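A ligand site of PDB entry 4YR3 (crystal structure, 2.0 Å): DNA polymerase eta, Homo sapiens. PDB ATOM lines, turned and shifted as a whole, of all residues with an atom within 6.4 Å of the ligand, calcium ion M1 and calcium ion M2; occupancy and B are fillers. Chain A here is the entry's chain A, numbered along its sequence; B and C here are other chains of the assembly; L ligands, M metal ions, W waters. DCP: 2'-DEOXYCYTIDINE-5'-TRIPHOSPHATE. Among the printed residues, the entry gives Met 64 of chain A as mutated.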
ATOM      1  N   ASP A  16       2.896  12.931  21.586  1.00  0.00           N
ATOM      2  CA  ASP A  16       1.697  12.316  21.045  1.00  0.00           C
ATOM      3  C   ASP A  16       1.780  10.773  20.922  1.00  0.00           C
ATOM      4  O   ASP A  16       2.686  10.258  20.288  1.00  0.00           O
ATOM      5  CB  ASP A  16       1.401  12.910  19.686  1.00  0.00           C
ATOM      6  CG  ASP A  16       0.269  12.197  18.992  1.00  0.00           C
ATOM      7  OD1 ASP A  16      -0.871  12.502  19.305  1.00  0.00           O
ATOM      8  OD2 ASP A  16       0.532  11.306  18.166  1.00  0.00           O
ATOM      9  N   MET A  17       0.845  10.034  21.511  1.00  0.00           N
ATOM     10  CA  MET A  17       0.903   8.568  21.487  1.00  0.00           C
ATOM     11  C   MET A  17       0.698   8.041  20.077  1.00  0.00           C
ATOM     12  O   MET A  17      -0.116   8.581  19.328  1.00  0.00           O
ATOM     13  CB  MET A  17      -0.155   7.963  22.429  1.00  0.00           C
ATOM     14  CG  MET A  17      -0.190   8.608  23.819  1.00  0.00           C
ATOM     15  SD  MET A  17       1.436   8.583  24.601  1.00  0.00           S
ATOM     16  CE  MET A  17       1.720   6.831  24.694  1.00  0.00           C
ATOM     17  N   ASP A  18       1.450   7.012  19.694  1.00  0.00           N
ATOM     18  CA  ASP A  18       1.279   6.404  18.381  1.00  0.00           C
ATOM     19  C   ASP A  18      -0.021   5.576  18.362  1.00  0.00           C
ATOM     20  O   ASP A  18      -0.275   4.843  19.320  1.00  0.00           O
ATOM     21  CB  ASP A  18       2.489   5.533  18.045  1.00  0.00           C
ATOM     22  CG  ASP A  18       3.791   6.329  17.980  1.00  0.00           C
ATOM     23  OD1 ASP A  18       3.738   7.529  17.636  1.00  0.00           O
ATOM     24  OD2 ASP A  18       4.865   5.767  18.271  1.00  0.00           O
ATOM     25  N   CYS A  19      -0.797   5.681  17.280  1.00  0.00           N
ATOM     26  CA  CYS A  19      -2.085   4.976  17.105  1.00  0.00           C
ATOM     27  C   CYS A  19      -2.722   4.572  18.440  1.00  0.00           C
ATOM     28  O   CYS A  19      -2.846   3.391  18.751  1.00  0.00           O
ATOM     29  CB  CYS A  19      -1.926   3.735  16.189  1.00  0.00           C
ATOM     30  SG  CYS A  19      -0.619   2.558  16.663  1.00  0.00           S
ATOM     31  N   PHE A  20      -3.072   5.574  19.242  1.00  0.00           N
ATOM     32  CA  PHE A  20      -3.279   5.368  20.682  1.00  0.00           C
ATOM     33  C   PHE A  20      -4.300   4.271  21.087  1.00  0.00           C
ATOM     34  O   PHE A  20      -3.976   3.381  21.897  1.00  0.00           O
ATOM     35  CB  PHE A  20      -3.679   6.702  21.341  1.00  0.00           C
ATOM     36  CG  PHE A  20      -3.807   6.607  22.836  1.00  0.00           C
ATOM     37  CD1 PHE A  20      -2.818   5.972  23.595  1.00  0.00           C
ATOM     38  CD2 PHE A  20      -4.919   7.124  23.486  1.00  0.00           C
ATOM     39  CE1 PHE A  20      -2.937   5.865  24.977  1.00  0.00           C
ATOM     40  CE2 PHE A  20      -5.034   7.039  24.871  1.00  0.00           C
ATOM     41  CZ  PHE A  20      -4.042   6.409  25.617  1.00  0.00           C
ATOM     42  N   PHE A  21      -5.523   4.334  20.548  1.00  0.00           N
ATOM     43  CA  PHE A  21      -6.548   3.385  20.992  1.00  0.00           C
ATOM     44  C   PHE A  21      -6.094   1.953  20.598  1.00  0.00           C
ATOM     45  O   PHE A  21      -6.305   0.969  21.334  1.00  0.00           O
ATOM     46  CB  PHE A  21      -7.941   3.684  20.387  1.00  0.00           C
ATOM     47  CG  PHE A  21      -8.642   4.911  20.973  1.00  0.00           C
ATOM     48  CD1 PHE A  21      -7.973   5.823  21.771  1.00  0.00           C
ATOM     49  CD2 PHE A  21      -9.983   5.135  20.690  1.00  0.00           C
ATOM     50  CE1 PHE A  21      -8.630   6.934  22.285  1.00  0.00           C
ATOM     51  CE2 PHE A  21     -10.651   6.238  21.207  1.00  0.00           C
ATOM     52  CZ  PHE A  21      -9.975   7.140  22.009  1.00  0.00           C
ATOM     53  N   VAL A  22      -5.443   1.869  19.434  1.00  0.00           N
ATOM     54  CA  VAL A  22      -4.920   0.595  18.980  1.00  0.00           C
ATOM     55  C   VAL A  22      -3.896   0.056  19.981  1.00  0.00           C
ATOM     56  O   VAL A  22      -4.015  -1.096  20.398  1.00  0.00           O
ATOM     57  CB  VAL A  22      -4.298   0.696  17.591  1.00  0.00           C
ATOM     58  CG1 VAL A  22      -3.446  -0.545  17.294  1.00  0.00           C
ATOM     59  CG2 VAL A  22      -5.404   0.862  16.541  1.00  0.00           C
ATOM     60  N   ILE A  51     -12.044   3.917  14.163  1.00  0.00           N
ATOM     61  CA  ILE A  51     -11.574   5.158  14.773  1.00  0.00           C
ATOM     62  C   ILE A  51     -10.092   5.156  15.123  1.00  0.00           C
ATOM     63  O   ILE A  51      -9.561   6.195  15.534  1.00  0.00           O
ATOM     64  CB  ILE A  51     -12.388   5.498  16.037  1.00  0.00           C
ATOM     65  CG1 ILE A  51     -12.179   4.452  17.141  1.00  0.00           C
ATOM     66  CG2 ILE A  51     -13.895   5.625  15.681  1.00  0.00           C
ATOM     67  CD1 ILE A  51     -12.910   4.825  18.459  1.00  0.00           C
ATOM     68  N   ALA A  52      -9.428   4.016  14.964  1.00  0.00           N
ATOM     69  CA  ALA A  52      -7.941   4.054  15.051  1.00  0.00           C
ATOM     70  C   ALA A  52      -7.307   2.909  14.292  1.00  0.00           C
ATOM     71  O   ALA A  52      -7.905   1.855  14.197  1.00  0.00           O
ATOM     72  CB  ALA A  52      -7.483   4.045  16.517  1.00  0.00           C
ATOM     73  N   VAL A  53      -6.092   3.097  13.765  1.00  0.00           N
ATOM     74  CA  VAL A  53      -5.489   2.152  12.819  1.00  0.00           C
ATOM     75  C   VAL A  53      -4.005   1.927  13.106  1.00  0.00           C
ATOM     76  O   VAL A  53      -3.239   2.894  13.197  1.00  0.00           O
ATOM     77  CB  VAL A  53      -5.609   2.657  11.371  1.00  0.00           C
ATOM     78  CG1 VAL A  53      -5.189   1.589  10.361  1.00  0.00           C
ATOM     79  CG2 VAL A  53      -7.028   3.132  11.062  1.00  0.00           C
ATOM     80  N   TYR A  55      -0.024   0.938  12.371  1.00  0.00           N
ATOM     81  CA  TYR A  55       0.787   1.335  11.214  1.00  0.00           C
ATOM     82  C   TYR A  55       0.848   0.234  10.144  1.00  0.00           C
ATOM     83  O   TYR A  55       0.780   0.514   8.915  1.00  0.00           O
ATOM     84  CB  TYR A  55       2.196   1.780  11.677  1.00  0.00           C
ATOM     85  CG  TYR A  55       2.097   3.206  12.200  1.00  0.00           C
ATOM     86  CD1 TYR A  55       1.653   3.465  13.495  1.00  0.00           C
ATOM     87  CD2 TYR A  55       2.377   4.281  11.376  1.00  0.00           C
ATOM     88  CE1 TYR A  55       1.495   4.768  13.946  1.00  0.00           C
ATOM     89  CE2 TYR A  55       2.253   5.597  11.823  1.00  0.00           C
ATOM     90  CZ  TYR A  55       1.815   5.832  13.117  1.00  0.00           C
ATOM     91  OH  TYR A  55       1.664   7.128  13.582  1.00  0.00           O
ATOM     92  N   ARG A  58      -2.196   0.642   8.187  1.00  0.00           N
ATOM     93  CA  ARG A  58      -2.054   1.841   7.365  1.00  0.00           C
ATOM     94  C   ARG A  58      -1.308   1.516   6.093  1.00  0.00           C
ATOM     95  O   ARG A  58      -1.564   2.124   5.052  1.00  0.00           O
ATOM     96  CB  ARG A  58      -1.329   2.953   8.117  1.00  0.00           C
ATOM     97  CG  ARG A  58      -2.115   3.519   9.273  1.00  0.00           C
ATOM     98  CD  ARG A  58      -1.355   4.601  10.027  1.00  0.00           C
ATOM     99  NE  ARG A  58      -1.892   4.739  11.378  1.00  0.00           N
ATOM    100  CZ  ARG A  58      -1.680   5.774  12.170  1.00  0.00           C
ATOM    101  NH1 ARG A  58      -0.922   6.791  11.757  1.00  0.00           N
ATOM    102  NH2 ARG A  58      -2.245   5.796  13.372  1.00  0.00           N
ATOM    103  N   MET A  64      -8.687   6.067   9.416  1.00  0.00           N
ATOM    104  CA  MET A  64      -9.785   6.588  10.226  1.00  0.00           C
ATOM    105  C   MET A  64     -11.037   6.911   9.401  1.00  0.00           C
ATOM    106  O   MET A  64     -10.939   7.332   8.249  1.00  0.00           O
ATOM    107  CB  MET A  64      -9.354   7.852  10.955  1.00  0.00           C
ATOM    108  CG  MET A  64      -8.989   7.638  12.402  1.00  0.00           C
ATOM    109  SD  MET A  64      -8.262   9.150  13.052  1.00  0.00           S
ATOM    110  CE  MET A  64      -7.122   8.488  14.265  1.00  0.00           C
ATOM    111  N   SER A  65     -12.198   6.742  10.040  1.00  0.00           N
ATOM    112  CA  SER A  65     -13.493   7.091   9.483  1.00  0.00           C
ATOM    113  C   SER A  65     -13.912   6.205   8.316  1.00  0.00           C
ATOM    114  O   SER A  65     -14.905   6.469   7.650  1.00  0.00           O
ATOM    115  CB  SER A  65     -13.515   8.551   9.060  1.00  0.00           C
ATOM    116  OG  SER A  65     -13.215   9.379  10.171  1.00  0.00           O
ATOM    117  N   LEU A  92     -16.016   5.333  26.316  1.00  0.00           N
ATOM    118  CA  LEU A  92     -14.580   5.505  26.092  1.00  0.00           C
ATOM    119  C   LEU A  92     -13.703   5.427  27.337  1.00  0.00           C
ATOM    120  O   LEU A  92     -12.550   5.823  27.308  1.00  0.00           O
ATOM    121  CB  LEU A  92     -14.340   6.846  25.388  1.00  0.00           C
ATOM    122  CG  LEU A  92     -15.098   6.960  24.056  1.00  0.00           C
ATOM    123  CD1 LEU A  92     -15.037   8.380  23.554  1.00  0.00           C
ATOM    124  CD2 LEU A  92     -14.527   6.009  23.015  1.00  0.00           C
ATOM    125  N   SER A 116      -5.140  16.765  24.282  1.00  0.00           N
ATOM    126  CA  SER A 116      -6.213  15.844  23.886  1.00  0.00           C
ATOM    127  C   SER A 116      -6.112  14.568  24.691  1.00  0.00           C
ATOM    128  O   SER A 116      -5.282  14.476  25.586  1.00  0.00           O
ATOM    129  CB  SER A 116      -6.119  15.532  22.399  1.00  0.00           C
ATOM    130  OG  SER A 116      -5.030  14.650  22.128  1.00  0.00           O
ATOM    131  N   ILE A 117      -6.922  13.561  24.357  1.00  0.00           N
ATOM    132  CA  ILE A 117      -6.820  12.301  25.091  1.00  0.00           C
ATOM    133  C   ILE A 117      -5.413  11.663  25.001  1.00  0.00           C
ATOM    134  O   ILE A 117      -5.000  10.955  25.913  1.00  0.00           O
ATOM    135  CB  ILE A 117      -7.865  11.277  24.618  1.00  0.00           C
ATOM    136  CG1 ILE A 117      -8.091  10.193  25.682  1.00  0.00           C
ATOM    137  CG2 ILE A 117      -7.477  10.672  23.274  1.00  0.00           C
ATOM    138  CD1 ILE A 117      -9.369   9.344  25.425  1.00  0.00           C
ATOM    139  N   ASP A 118      -4.650  11.922  23.941  1.00  0.00           N
ATOM    140  CA  ASP A 118      -3.359  11.231  23.782  1.00  0.00           C
ATOM    141  C   ASP A 118      -2.184  12.152  23.504  1.00  0.00           C
ATOM    142  O   ASP A 118      -1.120  11.702  23.053  1.00  0.00           O
ATOM    143  CB  ASP A 118      -3.452  10.169  22.682  1.00  0.00           C
ATOM    144  CG  ASP A 118      -3.204  10.746  21.290  1.00  0.00           C
ATOM    145  OD1 ASP A 118      -3.647  11.884  21.015  1.00  0.00           O
ATOM    146  OD2 ASP A 118      -2.548  10.063  20.457  1.00  0.00           O
ATOM    147  N   GLU A 119      -2.345  13.439  23.768  1.00  0.00           N
ATOM    148  CA  GLU A 119      -1.203  14.331  23.651  1.00  0.00           C
ATOM    149  C   GLU A 119      -1.176  15.468  24.645  1.00  0.00           C
ATOM    150  O   GLU A 119      -2.236  15.951  25.127  1.00  0.00           O
ATOM    151  CB  GLU A 119      -1.119  14.894  22.228  1.00  0.00           C
ATOM    152  CG  GLU A 119      -2.122  15.942  21.931  1.00  0.00           C
ATOM    153  CD  GLU A 119      -2.381  16.060  20.448  1.00  0.00           C
ATOM    154  OE1 GLU A 119      -1.789  16.954  19.811  1.00  0.00           O
ATOM    155  OE2 GLU A 119      -3.159  15.260  19.926  1.00  0.00           O
ATOM    156  N   LYS A 227       4.258  20.742  17.670  1.00  0.00           N
ATOM    157  CA  LYS A 227       3.218  19.915  17.055  1.00  0.00           C
ATOM    158  C   LYS A 227       3.578  19.520  15.608  1.00  0.00           C
ATOM    159  O   LYS A 227       3.437  18.350  15.225  1.00  0.00           O
ATOM    160  CB  LYS A 227       1.867  20.653  17.097  1.00  0.00           C
ATOM    161  CG  LYS A 227       0.711  19.929  16.417  1.00  0.00           C
ATOM    162  CD  LYS A 227       0.472  18.562  17.055  1.00  0.00           C
ATOM    163  CE  LYS A 227      -0.870  17.956  16.615  1.00  0.00           C
ATOM    164  NZ  LYS A 227      -0.983  16.548  17.057  1.00  0.00           N
ATOM    165  N   LYS A 234       7.144   9.759  12.386  1.00  0.00           N
ATOM    166  CA  LYS A 234       6.291   8.889  13.201  1.00  0.00           C
ATOM    167  C   LYS A 234       6.354   7.524  12.556  1.00  0.00           C
ATOM    168  O   LYS A 234       6.625   7.429  11.375  1.00  0.00           O
ATOM    169  CB  LYS A 234       4.844   9.411  13.249  1.00  0.00           C
ATOM    170  CG  LYS A 234       4.495  10.318  14.431  1.00  0.00           C
ATOM    171  CD  LYS A 234       2.992  10.622  14.478  1.00  0.00           C
ATOM    172  CE  LYS A 234       2.512  11.095  15.849  1.00  0.00           C
ATOM    173  NZ  LYS A 234       2.216   9.978  16.839  1.00  0.00           N
ATOM    174  N   PRO A 235       6.132   6.460  13.334  1.00  0.00           N
ATOM    175  CA  PRO A 235       5.933   6.401  14.792  1.00  0.00           C
ATOM    176  C   PRO A 235       7.224   6.206  15.600  1.00  0.00           C
ATOM    177  O   PRO A 235       8.284   5.971  15.021  1.00  0.00           O
ATOM    178  CB  PRO A 235       5.016   5.189  14.966  1.00  0.00           C
ATOM    179  CG  PRO A 235       5.457   4.262  13.847  1.00  0.00           C
ATOM    180  CD  PRO A 235       5.888   5.150  12.693  1.00  0.00           C
ATOM    181  P    DT B   8      -5.577  17.202  14.997  1.00  0.00           P
ATOM    182  OP1  DT B   8      -4.094  17.111  14.973  1.00  0.00           O
ATOM    183  OP2  DT B   8      -6.368  16.789  13.817  1.00  0.00           O
ATOM    184  O5'  DT B   8      -6.136  16.335  16.237  1.00  0.00           O
ATOM    185  C5'  DT B   8      -5.824  16.705  17.593  1.00  0.00           C
ATOM    186  C4'  DT B   8      -6.342  15.643  18.556  1.00  0.00           C
ATOM    187  O4'  DT B   8      -7.794  15.679  18.569  1.00  0.00           O
ATOM    188  C3'  DT B   8      -5.940  14.227  18.198  1.00  0.00           C
ATOM    189  O3'  DT B   8      -5.561  13.540  19.370  1.00  0.00           O
ATOM    190  C2'  DT B   8      -7.207  13.632  17.551  1.00  0.00           C
ATOM    191  C1'  DT B   8      -8.323  14.401  18.252  1.00  0.00           C
ATOM    192  N1   DT B   8      -9.569  14.592  17.404  1.00  0.00           N
ATOM    193  C2   DT B   8     -10.783  14.130  17.877  1.00  0.00           C
ATOM    194  O2   DT B   8     -10.913  13.563  18.946  1.00  0.00           O
ATOM    195  N3   DT B   8     -11.839  14.360  17.051  1.00  0.00           N
ATOM    196  C4   DT B   8     -11.837  14.973  15.821  1.00  0.00           C
ATOM    197  O4   DT B   8     -12.875  15.115  15.148  1.00  0.00           O
ATOM    198  C5   DT B   8     -10.552  15.437  15.371  1.00  0.00           C
ATOM    199  C7   DT B   8     -10.422  16.123  14.040  1.00  0.00           C
ATOM    200  C6   DT B   8      -9.482  15.217  16.172  1.00  0.00           C
ATOM    201  P    DG C   4     -22.152   9.066  11.895  1.00  0.00           P
ATOM    202  OP1  DG C   4     -23.546   8.854  12.329  1.00  0.00           O
ATOM    203  OP2  DG C   4     -21.693  10.386  11.420  1.00  0.00           O
ATOM    204  O5'  DG C   4     -21.273   8.714  13.173  1.00  0.00           O
ATOM    205  C5'  DG C   4     -21.287   7.376  13.688  1.00  0.00           C
ATOM    206  C4'  DG C   4     -20.810   7.355  15.137  1.00  0.00           C
ATOM    207  O4'  DG C   4     -19.418   7.762  15.206  1.00  0.00           O
ATOM    208  C3'  DG C   4     -21.553   8.275  16.100  1.00  0.00           C
ATOM    209  O3'  DG C   4     -21.547   7.678  17.377  1.00  0.00           O
ATOM    210  C2'  DG C   4     -20.693   9.535  16.068  1.00  0.00           C
ATOM    211  C1'  DG C   4     -19.301   8.930  15.997  1.00  0.00           C
ATOM    212  N9   DG C   4     -18.278   9.775  15.368  1.00  0.00           N
ATOM    213  C8   DG C   4     -18.436  10.653  14.321  1.00  0.00           C
ATOM    214  N7   DG C   4     -17.312  11.242  13.978  1.00  0.00           N
ATOM    215  C5   DG C   4     -16.366  10.701  14.838  1.00  0.00           C
ATOM    216  C6   DG C   4     -14.971  10.940  14.930  1.00  0.00           C
ATOM    217  O6   DG C   4     -14.276  11.717  14.255  1.00  0.00           O
ATOM    218  N1   DG C   4     -14.384  10.183  15.941  1.00  0.00           N
ATOM    219  C2   DG C   4     -15.064   9.302  16.753  1.00  0.00           C
ATOM    220  N2   DG C   4     -14.342   8.655  17.681  1.00  0.00           N
ATOM    221  N3   DG C   4     -16.357   9.061  16.665  1.00  0.00           N
ATOM    222  C4   DG C   4     -16.942   9.796  15.684  1.00  0.00           C
ATOM    223  P    DA C   5     -22.136   8.424  18.671  1.00  0.00           P
ATOM    224  OP1  DA C   5     -22.783   7.308  19.383  1.00  0.00           O
ATOM    225  OP2  DA C   5     -22.903   9.650  18.331  1.00  0.00           O
ATOM    226  O5'  DA C   5     -20.833   8.881  19.470  1.00  0.00           O
ATOM    227  C5'  DA C   5     -19.981   7.904  20.080  1.00  0.00           C
ATOM    228  C4'  DA C   5     -18.874   8.556  20.883  1.00  0.00           C
ATOM    229  O4'  DA C   5     -17.960   9.235  19.984  1.00  0.00           O
ATOM    230  C3'  DA C   5     -19.333   9.593  21.904  1.00  0.00           C
ATOM    231  O3'  DA C   5     -18.536   9.491  23.093  1.00  0.00           O
ATOM    232  C2'  DA C   5     -19.063  10.917  21.176  1.00  0.00           C
ATOM    233  C1'  DA C   5     -17.773  10.559  20.425  1.00  0.00           C
ATOM    234  N9   DA C   5     -17.514  11.416  19.278  1.00  0.00           N
ATOM    235  C8   DA C   5     -18.403  11.852  18.354  1.00  0.00           C
ATOM    236  N7   DA C   5     -17.868  12.614  17.423  1.00  0.00           N
ATOM    237  C5   DA C   5     -16.538  12.669  17.768  1.00  0.00           C
ATOM    238  C6   DA C   5     -15.428  13.317  17.198  1.00  0.00           C
ATOM    239  N6   DA C   5     -15.483  14.075  16.103  1.00  0.00           N
ATOM    240  N1   DA C   5     -14.245  13.149  17.809  1.00  0.00           N
ATOM    241  C2   DA C   5     -14.169  12.401  18.912  1.00  0.00           C
ATOM    242  N3   DA C   5     -15.131  11.750  19.541  1.00  0.00           N
ATOM    243  C4   DA C   5     -16.300  11.934  18.923  1.00  0.00           C
HETATM  244  N1  DCP L   1      -9.603   9.772  17.782  1.00  0.00           N
HETATM  245  C2  DCP L   1     -10.987   9.761  17.547  1.00  0.00           C
HETATM  246  N3  DCP L   1     -11.502  10.456  16.508  1.00  0.00           N
HETATM  247  C4  DCP L   1     -10.712  11.151  15.653  1.00  0.00           C
HETATM  248  C5  DCP L   1      -9.335  11.165  15.865  1.00  0.00           C
HETATM  249  C6  DCP L   1      -8.806  10.462  16.950  1.00  0.00           C
HETATM  250  O2  DCP L   1     -11.730   9.098  18.315  1.00  0.00           O
HETATM  251  N4  DCP L   1     -11.282  11.825  14.611  1.00  0.00           N
HETATM  252  C1' DCP L   1      -9.072   9.016  18.930  1.00  0.00           C
HETATM  253  C2' DCP L   1      -8.529   7.668  18.442  1.00  0.00           C
HETATM  254  C3' DCP L   1      -7.024   7.903  18.366  1.00  0.00           C
HETATM  255  C4' DCP L   1      -6.761   8.939  19.449  1.00  0.00           C
HETATM  256  O4' DCP L   1      -7.972   9.711  19.502  1.00  0.00           O
HETATM  257  O3' DCP L   1      -6.253   6.712  18.542  1.00  0.00           O
HETATM  258  C5' DCP L   1      -5.598   9.852  19.087  1.00  0.00           C
HETATM  259  O5' DCP L   1      -5.836  10.414  17.797  1.00  0.00           O
HETATM  260  PA  DCP L   1      -4.628  10.834  16.813  1.00  0.00           P
HETATM  261  O1A DCP L   1      -3.410  11.222  17.605  1.00  0.00           O
HETATM  262  O2A DCP L   1      -5.314  11.806  15.898  1.00  0.00           O
HETATM  263  O3A DCP L   1      -4.281   9.498  15.972  1.00  0.00           O
HETATM  264  PB  DCP L   1      -3.577   8.128  16.527  1.00  0.00           P
HETATM  265  O1B DCP L   1      -3.000   8.352  17.905  1.00  0.00           O
HETATM  266  O2B DCP L   1      -4.578   6.993  16.389  1.00  0.00           O
HETATM  267  O3B DCP L   1      -2.482   7.860  15.371  1.00  0.00           O
HETATM  268  PG  DCP L   1      -1.085   8.702  15.172  1.00  0.00           P
HETATM  269  O1G DCP L   1      -1.189   9.874  16.117  1.00  0.00           O
HETATM  270  O2G DCP L   1      -1.155   9.043  13.704  1.00  0.00           O
HETATM  271  O3G DCP L   1      -0.044   7.667  15.530  1.00  0.00           O
HETATM  272 CA    CA M   1      -1.567  10.102  18.371  1.00  0.00          CA
HETATM  273 CA    CA M   2      -3.082  13.135  19.119  1.00  0.00          CA
HETATM  274  O   HOH W   1     -12.910   8.595  20.782  1.00  0.00           O
HETATM  275  O   HOH W   2      -9.360  12.954  12.647  1.00  0.00           O
HETATM  276  O   HOH W   3      -2.558  14.109  16.966  1.00  0.00           O
HETATM  277  O   HOH W   4      -1.292  12.309  14.889  1.00  0.00           O
HETATM  278  O   HOH W   5      -5.212   5.850  14.050  1.00  0.00           O
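Calcium ion M1 is bound by O1A of the ligand, O1G of the ligand, OD2 of Asp 118, O1B of the ligand, O of Met 17, OD2 of Asp 16 and OD1 of Asp 16.
Water W5 lies within hydrogen-bond range of O2B of the ligand (2.7 Å), N of Val 53 (2.9 Å) and NH2 of Arg 58 (3.0 Å). Water W1 bridges O2 of the ligand (2.8 Å) and N2 of DG 4 of chain C (3.4 Å).
An oxygen (O3G) of the ligand is in hydrogen-bond range of the side-chain hydroxyl (OH) of Tyr 55 (2.6 Å). O6 of DG 4 of chain C lies within hydrogen-bond range of a nitrogen (N4) of the ligand. The backbone NH (N) of Cys 19 lies within hydrogen-bond range of an oxygen (O3G) of the ligand (2.8 Å). The guanidinium group (NH1) of Arg 58 lies within salt-bridge range of an oxygen (O2G) of the ligand, 3.0 Å away. O3' of the ligand is in hydrogen-bond range of N of Phe 20 (3.5 Å). N of Phe 21 lies within hydrogen-bond range of O3' of the ligand, at 3.2 Å. An oxygen (O3G) of the ligand lies within salt-bridge range of the side-chain amino group (NZ) of Lys 234 (3.5 Å).
Ser 116 touches calcium ion M2.
Asp 18 touches the ligand. Ile 51 touches the ligand. CB of Ala 52 touches O3' of the ligand, at 3.6 Å. Met 64 touches the ligand. Ile 117 touches the ligand (CG2 to O4', 3.9 Å). Hydrophobic or aromatic side chains within 4 Å of the ligand: Phe 20, Phe 21, Ala 52, Tyr 55, Met 64 and Ile 117. Of the 25 residues printed, 16 come within 4 Å of the ligand. The nearest printed residue that does not touch the ligand is DA 5 of chain C (4.1 Å).
OG of Ser 116 sits close to N of Glu 119 (3.4 Å). The side-chain amino group (NZ) of Lys 227 lies within salt-bridge range of the side-chain carboxylate (OE1) of Glu 119, 2.9 Å away. The backbone NH (N) of Asp 118 lies close to the side-chain hydroxyl (OG) of Ser 116 (3.3 Å). The side-chain amino group of Lys 234 sits at hydrogen-bond distance from the backbone carbonyl oxygen of Asp 16, at 3.5 Å. O3' of DT 8 of chain B sits close to the side-chain hydroxyl (OG) of Ser 116, at 3.0 Å. The guanidinium group (NH1) of Arg 58 lies within hydrogen-bond range of the side-chain hydroxyl (OH) of Tyr 55. The guanidinium group (NE) of Arg 58 sits at hydrogen-bond distance from the backbone carbonyl oxygen (O) of Val 53 (2.9 Å). OD1 of Asp 18 is in salt-bridge range of NZ of Lys 234.
The side-chain carboxylate (OE2) of Glu 119 binds calcium ion M2 (2.3 Å). OD1 of Asp 16 is bound to calcium ion M2. Calcium ion M2 is bound by OD1 of Asp 118. Calcium ion M2 is bound by water W3. Calcium ion M2 is bound by an oxygen (O1A) of the ligand. Calcium ion M2 is bound by O3' of DT 8 of chain B, at 2.5 Å. Calcium ion M2 has six donor atoms within binding distance.
Within 4 Å of calcium ion M1: Asp 16, Met 17 and Asp 118.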
